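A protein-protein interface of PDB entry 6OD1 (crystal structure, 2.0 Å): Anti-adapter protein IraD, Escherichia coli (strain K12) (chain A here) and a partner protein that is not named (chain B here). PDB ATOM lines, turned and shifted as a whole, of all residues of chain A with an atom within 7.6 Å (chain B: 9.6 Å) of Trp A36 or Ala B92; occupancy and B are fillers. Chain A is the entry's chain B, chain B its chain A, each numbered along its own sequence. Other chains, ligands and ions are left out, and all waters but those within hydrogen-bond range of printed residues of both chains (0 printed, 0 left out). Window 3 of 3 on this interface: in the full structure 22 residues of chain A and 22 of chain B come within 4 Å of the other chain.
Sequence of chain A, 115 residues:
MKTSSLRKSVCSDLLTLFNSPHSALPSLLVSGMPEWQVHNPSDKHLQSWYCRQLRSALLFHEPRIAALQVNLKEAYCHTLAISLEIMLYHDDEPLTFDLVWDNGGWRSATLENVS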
ATOM      1  N   LEU A  28     -20.621  34.977  10.669  1.00  0.00           N
ATOM      2  CA  LEU A  28     -21.551  33.879  10.912  1.00  0.00           C
ATOM      3  C   LEU A  28     -22.981  34.237  10.504  1.00  0.00           C
ATOM      4  O   LEU A  28     -23.704  33.401   9.939  1.00  0.00           O
ATOM      5  CB  LEU A  28     -21.497  33.507  12.397  1.00  0.00           C
ATOM      6  CG  LEU A  28     -22.035  32.160  12.869  1.00  0.00           C
ATOM      7  CD1 LEU A  28     -21.323  31.031  12.179  1.00  0.00           C
ATOM      8  CD2 LEU A  28     -21.880  32.047  14.387  1.00  0.00           C
ATOM      9  N   SER A  31     -23.052  35.697   6.141  1.00  0.00           N
ATOM     10  CA  SER A  31     -22.839  34.670   5.125  1.00  0.00           C
ATOM     11  C   SER A  31     -22.988  33.252   5.653  1.00  0.00           C
ATOM     12  O   SER A  31     -23.484  32.390   4.923  1.00  0.00           O
ATOM     13  CB  SER A  31     -21.446  34.824   4.479  1.00  0.00           C
ATOM     14  OG  SER A  31     -20.472  35.261   5.418  1.00  0.00           O
ATOM     15  N   GLY A  32     -22.606  32.993   6.905  1.00  0.00           N
ATOM     16  CA  GLY A  32     -22.621  31.645   7.437  1.00  0.00           C
ATOM     17  C   GLY A  32     -23.973  30.968   7.348  1.00  0.00           C
ATOM     18  O   GLY A  32     -24.109  29.919   6.705  1.00  0.00           O
ATOM     19  N   MET A  33     -24.981  31.572   7.978  1.00  0.00           N
ATOM     20  CA  MET A  33     -26.327  31.000   7.951  1.00  0.00           C
ATOM     21  C   MET A  33     -26.879  30.801   6.542  1.00  0.00           C
ATOM     22  O   MET A  33     -27.404  29.708   6.265  1.00  0.00           O
ATOM     23  CB  MET A  33     -27.264  31.865   8.797  1.00  0.00           C
ATOM     24  CG  MET A  33     -28.691  31.341   8.846  1.00  0.00           C
ATOM     25  SD  MET A  33     -28.855  29.917   9.959  1.00  0.00           S
ATOM     26  CE  MET A  33     -30.642  29.826  10.165  1.00  0.00           C
ATOM     27  N   PRO A  34     -26.823  31.776   5.618  1.00  0.00           N
ATOM     28  CA  PRO A  34     -27.298  31.478   4.251  1.00  0.00           C
ATOM     29  C   PRO A  34     -26.592  30.296   3.610  1.00  0.00           C
ATOM     30  O   PRO A  34     -27.247  29.445   2.990  1.00  0.00           O
ATOM     31  CB  PRO A  34     -27.015  32.779   3.480  1.00  0.00           C
ATOM     32  CG  PRO A  34     -26.961  33.819   4.482  1.00  0.00           C
ATOM     33  CD  PRO A  34     -26.453  33.195   5.762  1.00  0.00           C
ATOM     34  N   GLU A  35     -25.265  30.221   3.738  1.00  0.00           N
ATOM     35  CA  GLU A  35     -24.513  29.141   3.104  1.00  0.00           C
ATOM     36  C   GLU A  35     -24.733  27.801   3.800  1.00  0.00           C
ATOM     37  O   GLU A  35     -24.562  26.750   3.171  1.00  0.00           O
ATOM     38  CB  GLU A  35     -23.024  29.495   3.074  1.00  0.00           C
ATOM     39  CG  GLU A  35     -22.638  30.465   1.953  1.00  0.00           C
ATOM     40  CD  GLU A  35     -21.536  31.435   2.359  1.00  0.00           C
ATOM     41  OE1 GLU A  35     -20.814  31.143   3.336  1.00  0.00           O
ATOM     42  OE2 GLU A  35     -21.392  32.492   1.705  1.00  0.00           O
ATOM     43  N   TRP A  36     -25.114  27.821   5.078  1.00  0.00           N
ATOM     44  CA  TRP A  36     -25.464  26.598   5.794  1.00  0.00           C
ATOM     45  C   TRP A  36     -26.804  26.037   5.324  1.00  0.00           C
ATOM     46  O   TRP A  36     -26.960  24.819   5.181  1.00  0.00           O
ATOM     47  CB  TRP A  36     -25.496  26.881   7.303  1.00  0.00           C
ATOM     48  CG  TRP A  36     -25.744  25.660   8.135  1.00  0.00           C
ATOM     49  CD1 TRP A  36     -26.943  25.240   8.645  1.00  0.00           C
ATOM     50  CD2 TRP A  36     -24.773  24.697   8.544  1.00  0.00           C
ATOM     51  NE1 TRP A  36     -26.775  24.069   9.347  1.00  0.00           N
ATOM     52  CE2 TRP A  36     -25.451  23.713   9.300  1.00  0.00           C
ATOM     53  CE3 TRP A  36     -23.395  24.564   8.340  1.00  0.00           C
ATOM     54  CZ2 TRP A  36     -24.798  22.616   9.856  1.00  0.00           C
ATOM     55  CZ3 TRP A  36     -22.747  23.475   8.893  1.00  0.00           C
ATOM     56  CH2 TRP A  36     -23.450  22.512   9.641  1.00  0.00           C
ATOM     57  N   GLN A  37     -27.784  26.908   5.071  1.00  0.00           N
ATOM     58  CA  GLN A  37     -29.103  26.439   4.656  1.00  0.00           C
ATOM     59  C   GLN A  37     -29.102  25.799   3.272  1.00  0.00           C
ATOM     60  O   GLN A  37     -30.029  25.043   2.956  1.00  0.00           O
ATOM     61  CB  GLN A  37     -30.115  27.593   4.686  1.00  0.00           C
ATOM     62  CG  GLN A  37     -30.290  28.275   6.051  1.00  0.00           C
ATOM     63  CD  GLN A  37     -31.122  27.469   7.051  1.00  0.00           C
ATOM     64  OE1 GLN A  37     -32.178  27.920   7.505  1.00  0.00           O
ATOM     65  NE2 GLN A  37     -30.634  26.283   7.416  1.00  0.00           N
ATOM     66  N   VAL A  38     -28.099  26.073   2.432  1.00  0.00           N
ATOM     67  CA  VAL A  38     -28.114  25.454   1.107  1.00  0.00           C
ATOM     68  C   VAL A  38     -27.702  23.990   1.201  1.00  0.00           C
ATOM     69  O   VAL A  38     -28.166  23.157   0.413  1.00  0.00           O
ATOM     70  CB  VAL A  38     -27.233  26.239   0.108  1.00  0.00           C
ATOM     71  CG1 VAL A  38     -25.763  26.181   0.484  1.00  0.00           C
ATOM     72  CG2 VAL A  38     -27.428  25.706  -1.309  1.00  0.00           C
ATOM     73  N   HIS A  39     -26.887  23.641   2.199  1.00  0.00           N
ATOM     74  CA  HIS A  39     -26.274  22.327   2.305  1.00  0.00           C
ATOM     75  C   HIS A  39     -26.841  21.477   3.436  1.00  0.00           C
ATOM     76  O   HIS A  39     -26.418  20.327   3.598  1.00  0.00           O
ATOM     77  CB  HIS A  39     -24.754  22.473   2.489  1.00  0.00           C
ATOM     78  CG  HIS A  39     -24.065  23.186   1.363  1.00  0.00           C
ATOM     79  ND1 HIS A  39     -24.348  22.939   0.037  1.00  0.00           N
ATOM     80  CD2 HIS A  39     -23.094  24.132   1.369  1.00  0.00           C
ATOM     81  CE1 HIS A  39     -23.587  23.704  -0.726  1.00  0.00           C
ATOM     82  NE2 HIS A  39     -22.814  24.434   0.056  1.00  0.00           N
ATOM     83  N   ASN A  40     -27.795  21.990   4.208  1.00  0.00           N
ATOM     84  CA  ASN A  40     -28.257  21.290   5.402  1.00  0.00           C
ATOM     85  C   ASN A  40     -29.760  21.457   5.589  1.00  0.00           C
ATOM     86  O   ASN A  40     -30.306  22.537   5.311  1.00  0.00           O
ATOM     87  CB  ASN A  40     -27.531  21.800   6.659  1.00  0.00           C
ATOM     88  CG  ASN A  40     -26.038  21.568   6.596  1.00  0.00           C
ATOM     89  OD1 ASN A  40     -25.272  22.470   6.262  1.00  0.00           O
ATOM     90  ND2 ASN A  40     -25.619  20.348   6.899  1.00  0.00           N
ATOM     91  N   PRO A  41     -30.446  20.421   6.070  1.00  0.00           N
ATOM     92  CA  PRO A  41     -31.889  20.536   6.295  1.00  0.00           C
ATOM     93  C   PRO A  41     -32.188  21.611   7.325  1.00  0.00           C
ATOM     94  O   PRO A  41     -31.418  21.823   8.264  1.00  0.00           O
ATOM     95  CB  PRO A  41     -32.278  19.148   6.806  1.00  0.00           C
ATOM     96  CG  PRO A  41     -31.206  18.226   6.238  1.00  0.00           C
ATOM     97  CD  PRO A  41     -29.952  19.054   6.314  1.00  0.00           C
ATOM     98  N   SER A  42     -33.314  22.296   7.126  1.00  0.00           N
ATOM     99  CA  SER A  42     -33.700  23.391   8.008  1.00  0.00           C
ATOM    100  C   SER A  42     -34.088  22.862   9.385  1.00  0.00           C
ATOM    101  O   SER A  42     -34.617  21.756   9.532  1.00  0.00           O
ATOM    102  CB  SER A  42     -34.857  24.193   7.400  1.00  0.00           C
ATOM    103  OG  SER A  42     -36.075  23.466   7.428  1.00  0.00           O
ATOM    104  N   ASP A  43     -33.813  23.666  10.406  1.00  0.00           N
ATOM    105  CA  ASP A  43     -34.034  23.244  11.778  1.00  0.00           C
ATOM    106  C   ASP A  43     -34.621  24.409  12.562  1.00  0.00           C
ATOM    107  O   ASP A  43     -34.068  25.512  12.555  1.00  0.00           O
ATOM    108  CB  ASP A  43     -32.725  22.749  12.403  1.00  0.00           C
ATOM    109  CG  ASP A  43     -32.914  22.196  13.796  1.00  0.00           C
ATOM    110  OD1 ASP A  43     -33.365  22.950  14.678  1.00  0.00           O
ATOM    111  OD2 ASP A  43     -32.610  21.005  14.013  1.00  0.00           O
ATOM    112  N   LEU A  46     -32.172  26.034  15.008  1.00  0.00           N
ATOM    113  CA  LEU A  46     -31.160  26.884  14.402  1.00  0.00           C
ATOM    114  C   LEU A  46     -31.773  28.188  13.915  1.00  0.00           C
ATOM    115  O   LEU A  46     -31.195  29.263  14.104  1.00  0.00           O
ATOM    116  CB  LEU A  46     -30.467  26.153  13.260  1.00  0.00           C
ATOM    117  CG  LEU A  46     -29.226  26.868  12.736  1.00  0.00           C
ATOM    118  CD1 LEU A  46     -28.097  26.760  13.725  1.00  0.00           C
ATOM    119  CD2 LEU A  46     -28.854  26.243  11.403  1.00  0.00           C
ATOM    120  N   ILE B  59     -15.931  28.553  22.733  1.00  0.00           N
ATOM    121  CA  ILE B  59     -15.570  27.343  22.015  1.00  0.00           C
ATOM    122  C   ILE B  59     -14.060  27.206  21.901  1.00  0.00           C
ATOM    123  O   ILE B  59     -13.489  26.192  22.312  1.00  0.00           O
ATOM    124  CB  ILE B  59     -16.268  27.308  20.646  1.00  0.00           C
ATOM    125  CG1 ILE B  59     -17.776  27.163  20.881  1.00  0.00           C
ATOM    126  CG2 ILE B  59     -15.722  26.159  19.775  1.00  0.00           C
ATOM    127  CD1 ILE B  59     -18.591  27.275  19.635  1.00  0.00           C
ATOM    128  N   LEU B  67     -16.678  22.652  22.634  1.00  0.00           N
ATOM    129  CA  LEU B  67     -17.619  21.662  22.123  1.00  0.00           C
ATOM    130  C   LEU B  67     -17.239  20.256  22.564  1.00  0.00           C
ATOM    131  O   LEU B  67     -18.118  19.426  22.821  1.00  0.00           O
ATOM    132  CB  LEU B  67     -17.704  21.727  20.599  1.00  0.00           C
ATOM    133  CG  LEU B  67     -18.392  22.967  20.033  1.00  0.00           C
ATOM    134  CD1 LEU B  67     -18.005  23.105  18.570  1.00  0.00           C
ATOM    135  CD2 LEU B  67     -19.912  22.919  20.214  1.00  0.00           C
ATOM    136  N   THR B  88     -16.794  32.246  17.216  1.00  0.00           N
ATOM    137  CA  THR B  88     -16.630  31.331  16.085  1.00  0.00           C
ATOM    138  C   THR B  88     -17.220  31.925  14.811  1.00  0.00           C
ATOM    139  O   THR B  88     -18.133  32.763  14.838  1.00  0.00           O
ATOM    140  CB  THR B  88     -17.298  29.979  16.357  1.00  0.00           C
ATOM    141  OG1 THR B  88     -17.089  29.095  15.243  1.00  0.00           O
ATOM    142  CG2 THR B  88     -18.797  30.165  16.541  1.00  0.00           C
ATOM    143  N   GLU B  89     -16.696  31.461  13.679  1.00  0.00           N
ATOM    144  CA  GLU B  89     -17.227  31.798  12.363  1.00  0.00           C
ATOM    145  C   GLU B  89     -17.761  30.571  11.634  1.00  0.00           C
ATOM    146  O   GLU B  89     -18.083  30.659  10.446  1.00  0.00           O
ATOM    147  CB  GLU B  89     -16.156  32.482  11.508  1.00  0.00           C
ATOM    148  CG  GLU B  89     -15.915  33.937  11.852  1.00  0.00           C
ATOM    149  CD  GLU B  89     -14.463  34.333  11.686  1.00  0.00           C
ATOM    150  OE1 GLU B  89     -13.788  33.757  10.807  1.00  0.00           O
ATOM    151  OE2 GLU B  89     -13.992  35.210  12.441  1.00  0.00           O
ATOM    152  N   ASN B  90     -17.873  29.435  12.317  1.00  0.00           N
ATOM    153  CA  ASN B  90     -18.247  28.170  11.700  1.00  0.00           C
ATOM    154  C   ASN B  90     -19.639  27.763  12.173  1.00  0.00           C
ATOM    155  O   ASN B  90     -19.826  27.461  13.358  1.00  0.00           O
ATOM    156  CB  ASN B  90     -17.228  27.088  12.056  1.00  0.00           C
ATOM    157  CG  ASN B  90     -17.503  25.780  11.354  1.00  0.00           C
ATOM    158  OD1 ASN B  90     -18.441  25.665  10.564  1.00  0.00           O
ATOM    159  ND2 ASN B  90     -16.677  24.781  11.633  1.00  0.00           N
ATOM    160  N   MET B  91     -20.598  27.712  11.235  1.00  0.00           N
ATOM    161  CA  MET B  91     -21.961  27.315  11.590  1.00  0.00           C
ATOM    162  C   MET B  91     -22.028  25.890  12.141  1.00  0.00           C
ATOM    163  O   MET B  91     -22.900  25.588  12.969  1.00  0.00           O
ATOM    164  CB  MET B  91     -22.897  27.468  10.388  1.00  0.00           C
ATOM    165  CG  MET B  91     -23.578  28.831  10.326  1.00  0.00           C
ATOM    166  SD  MET B  91     -24.644  29.175  11.775  1.00  0.00           S
ATOM    167  CE  MET B  91     -26.141  28.380  11.237  1.00  0.00           C
ATOM    168  N   ALA B  92     -21.131  24.998  11.697  1.00  0.00           N
ATOM    169  CA  ALA B  92     -21.107  23.646  12.252  1.00  0.00           C
ATOM    170  C   ALA B  92     -20.911  23.674  13.766  1.00  0.00           C
ATOM    171  O   ALA B  92     -21.459  22.828  14.480  1.00  0.00           O
ATOM    172  CB  ALA B  92     -20.019  22.805  11.577  1.00  0.00           C
ATOM    173  N   ASP B  93     -20.137  24.639  14.274  1.00  0.00           N
ATOM    174  CA  ASP B  93     -20.007  24.811  15.722  1.00  0.00           C
ATOM    175  C   ASP B  93     -21.355  25.112  16.363  1.00  0.00           C
ATOM    176  O   ASP B  93     -21.712  24.543  17.405  1.00  0.00           O
ATOM    177  CB  ASP B  93     -19.022  25.943  16.042  1.00  0.00           C
ATOM    178  CG  ASP B  93     -17.570  25.559  15.775  1.00  0.00           C
ATOM    179  OD1 ASP B  93     -17.301  24.373  15.507  1.00  0.00           O
ATOM    180  OD2 ASP B  93     -16.698  26.453  15.839  1.00  0.00           O
ATOM    181  N   ILE B  94     -22.106  26.035  15.763  1.00  0.00           N
ATOM    182  CA  ILE B  94     -23.398  26.432  16.314  1.00  0.00           C
ATOM    183  C   ILE B  94     -24.344  25.237  16.336  1.00  0.00           C
ATOM    184  O   ILE B  94     -24.940  24.902  17.371  1.00  0.00           O
ATOM    185  CB  ILE B  94     -23.986  27.593  15.492  1.00  0.00           C
ATOM    186  CG1 ILE B  94     -23.020  28.792  15.466  1.00  0.00           C
ATOM    187  CG2 ILE B  94     -25.396  27.932  15.982  1.00  0.00           C
ATOM    188  CD1 ILE B  94     -22.497  29.209  16.877  1.00  0.00           C
ATOM    189  N   ALA B  95     -24.496  24.586  15.184  1.00  0.00           N
ATOM    190  CA  ALA B  95     -25.365  23.419  15.073  1.00  0.00           C
ATOM    191  C   ALA B  95     -24.968  22.337  16.067  1.00  0.00           C
ATOM    192  O   ALA B  95     -25.835  21.690  16.664  1.00  0.00           O
ATOM    193  CB  ALA B  95     -25.332  22.870  13.640  1.00  0.00           C
ATOM    194  N   LYS B  96     -23.666  22.133  16.271  1.00  0.00           N
ATOM    195  CA  LYS B  96     -23.244  21.086  17.195  1.00  0.00           C
ATOM    196  C   LYS B  96     -23.597  21.449  18.633  1.00  0.00           C
ATOM    197  O   LYS B  96     -24.013  20.582  19.412  1.00  0.00           O
ATOM    198  CB  LYS B  96     -21.744  20.815  17.054  1.00  0.00           C
ATOM    199  CG  LYS B  96     -21.218  19.758  18.025  1.00  0.00           C
ATOM    200  CD  LYS B  96     -19.907  19.135  17.558  1.00  0.00           C
ATOM    201  CE  LYS B  96     -19.151  18.522  18.738  1.00  0.00           C
ATOM    202  NZ  LYS B  96     -17.795  18.022  18.363  1.00  0.00           N
ATOM    203  N   ALA B  97     -23.446  22.724  19.006  1.00  0.00           N
ATOM    204  CA  ALA B  97     -23.784  23.122  20.363  1.00  0.00           C
ATOM    205  C   ALA B  97     -25.282  22.988  20.617  1.00  0.00           C
ATOM    206  O   ALA B  97     -25.698  22.547  21.696  1.00  0.00           O
ATOM    207  CB  ALA B  97     -23.316  24.556  20.621  1.00  0.00           C
ATOM    208  N   LEU B  98     -26.110  23.349  19.631  1.00  0.00           N
ATOM    209  CA  LEU B  98     -27.556  23.314  19.831  1.00  0.00           C
ATOM    210  C   LEU B  98     -28.075  21.880  19.873  1.00  0.00           C
ATOM    211  O   LEU B  98     -29.003  21.576  20.632  1.00  0.00           O
ATOM    212  CB  LEU B  98     -28.264  24.121  18.738  1.00  0.00           C
ATOM    213  CG  LEU B  98     -28.100  25.653  18.795  1.00  0.00           C
ATOM    214  CD1 LEU B  98     -28.762  26.317  17.585  1.00  0.00           C
ATOM    215  CD2 LEU B  98     -28.646  26.240  20.091  1.00  0.00           C
ATOM    216  N   ARG B  99     -27.500  20.991  19.055  1.00  0.00           N
ATOM    217  CA  ARG B  99     -27.793  19.564  19.171  1.00  0.00           C
ATOM    218  C   ARG B  99     -27.462  19.039  20.571  1.00  0.00           C
ATOM    219  O   ARG B  99     -28.265  18.327  21.187  1.00  0.00           O
ATOM    220  CB  ARG B  99     -27.006  18.798  18.108  1.00  0.00           C
ATOM    221  CG  ARG B  99     -27.539  17.415  17.783  1.00  0.00           C
ATOM    222  CD  ARG B  99     -27.134  16.996  16.366  1.00  0.00           C
ATOM    223  NE  ARG B  99     -25.703  17.188  16.111  1.00  0.00           N
ATOM    224  CZ  ARG B  99     -25.199  18.035  15.212  1.00  0.00           C
ATOM    225  NH1 ARG B  99     -26.006  18.782  14.469  1.00  0.00           N
ATOM    226  NH2 ARG B  99     -23.882  18.136  15.054  1.00  0.00           N
ATOM    227  N   LEU B 100     -26.280  19.386  21.090  1.00  0.00           N
ATOM    228  CA  LEU B 100     -25.834  18.831  22.362  1.00  0.00           C
ATOM    229  C   LEU B 100     -26.673  19.333  23.531  1.00  0.00           C
ATOM    230  O   LEU B 100     -26.779  18.643  24.553  1.00  0.00           O
ATOM    231  CB  LEU B 100     -24.357  19.161  22.585  1.00  0.00           C
ATOM    232  CG  LEU B 100     -23.438  18.394  21.624  1.00  0.00           C
ATOM    233  CD1 LEU B 100     -21.996  18.885  21.711  1.00  0.00           C
ATOM    234  CD2 LEU B 100     -23.534  16.891  21.876  1.00  0.00           C
ATOM    235  N   VAL B 105     -26.090  29.971  22.354  1.00  0.00           N
ATOM    236  CA  VAL B 105     -24.735  30.309  21.934  1.00  0.00           C
ATOM    237  C   VAL B 105     -24.779  31.796  21.607  1.00  0.00           C
ATOM    238  O   VAL B 105     -25.406  32.200  20.623  1.00  0.00           O
ATOM    239  CB  VAL B 105     -24.273  29.481  20.729  1.00  0.00           C
ATOM    240  CG1 VAL B 105     -22.762  29.649  20.472  1.00  0.00           C
ATOM    241  CG2 VAL B 105     -24.605  27.985  20.920  1.00  0.00           C
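The side-chain hydroxyl of Thr B88 lies within hydrogen-bond range of the backbone NH of Asn B90, at 3.0 Å.
The side-chain carboxylate of Asp B93 is in hydrogen-bond range of the side-chain hydroxyl of Thr B88.
The side-chain amide oxygen of Asn B90 sits at hydrogen-bond distance from the backbone NH of Ala B92 (3.0 Å).
The backbone NH of Met A33 sits at hydrogen-bond distance from the backbone carbonyl oxygen of Leu A28, at 3.0 Å.
O of Trp A36 lies close to OD1 of Asn A40 (3.1 Å).
N of Leu A46 lies within hydrogen-bond range of OD1 of Asp A43.
Among the printed residues, pairs that only touch across the chains: Leu A28 with Thr B88 (3.8 Å), Leu A28 with Glu B89 (3.6 Å), Leu A28 with Asn B90 (3.7 Å), Leu A28 with Met B91 (3.5 Å), Leu A28 with Ile B94 (3.6 Å), Gly A32 with Met B91 (3.7 Å), Met A33 with Met B91 (3.4 Å), Trp A36 with Met B91 (3.6 Å), Trp A36 with Ala B92 (3.6 Å), Trp A36 with Ala B95 (3.8 Å), Leu A46 with Met B91 (3.5 Å), Leu A46 with Ile B94 (3.7 Å) and Leu A46 with Leu B98 (3.9 Å).
Of chain B, only Met B91, Ala B92 and Ala B95 come within 4 Å of Trp A36.
Pro A41 touches none of the printed residues of chain B.
Printed residues of chain A within 4 Å of Thr B88: Leu A28.
Printed residues of chain A within 4 Å of Met B91: Leu A28 (3.5 Å), Gly A32 (3.7 Å), Met A33 (3.4 Å), Trp A36 (3.6 Å) and Leu A46 (3.5 Å).
Ala B92 touches just one residue of chain A: Trp A36.
Of the printed residues of chain A, Ile B94 touches Leu A28 and Leu A46.
Printed residues of chain A within 4 Å of Leu B98: Leu A46.
The nearest residue of chain B that does not touch Trp A36 is Asn B90 (5.1 Å).
The nearest printed residue of chain A that does not touch Glu B89 is Gly A32 (5.5 Å).
Printed residues of chain A that touch a printed residue of chain B: Leu A28, Gly A32, Met A33, Trp A36 and Leu A46.
Hydrophobic or aromatic side chains of chain A within 4 Å of the printed part of chain B: Leu A28, Met A33, Trp A36 and Leu A46.
Of the 16 printed residues of chain B, 8 touch a printed residue of chain A.
Among the printed residues, 13 pairs touch across the chains.
Among the printed residues, no Asp or Glu carboxylate lies within 4 Å of a Lys or Arg side-chain nitrogen of the other chain.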
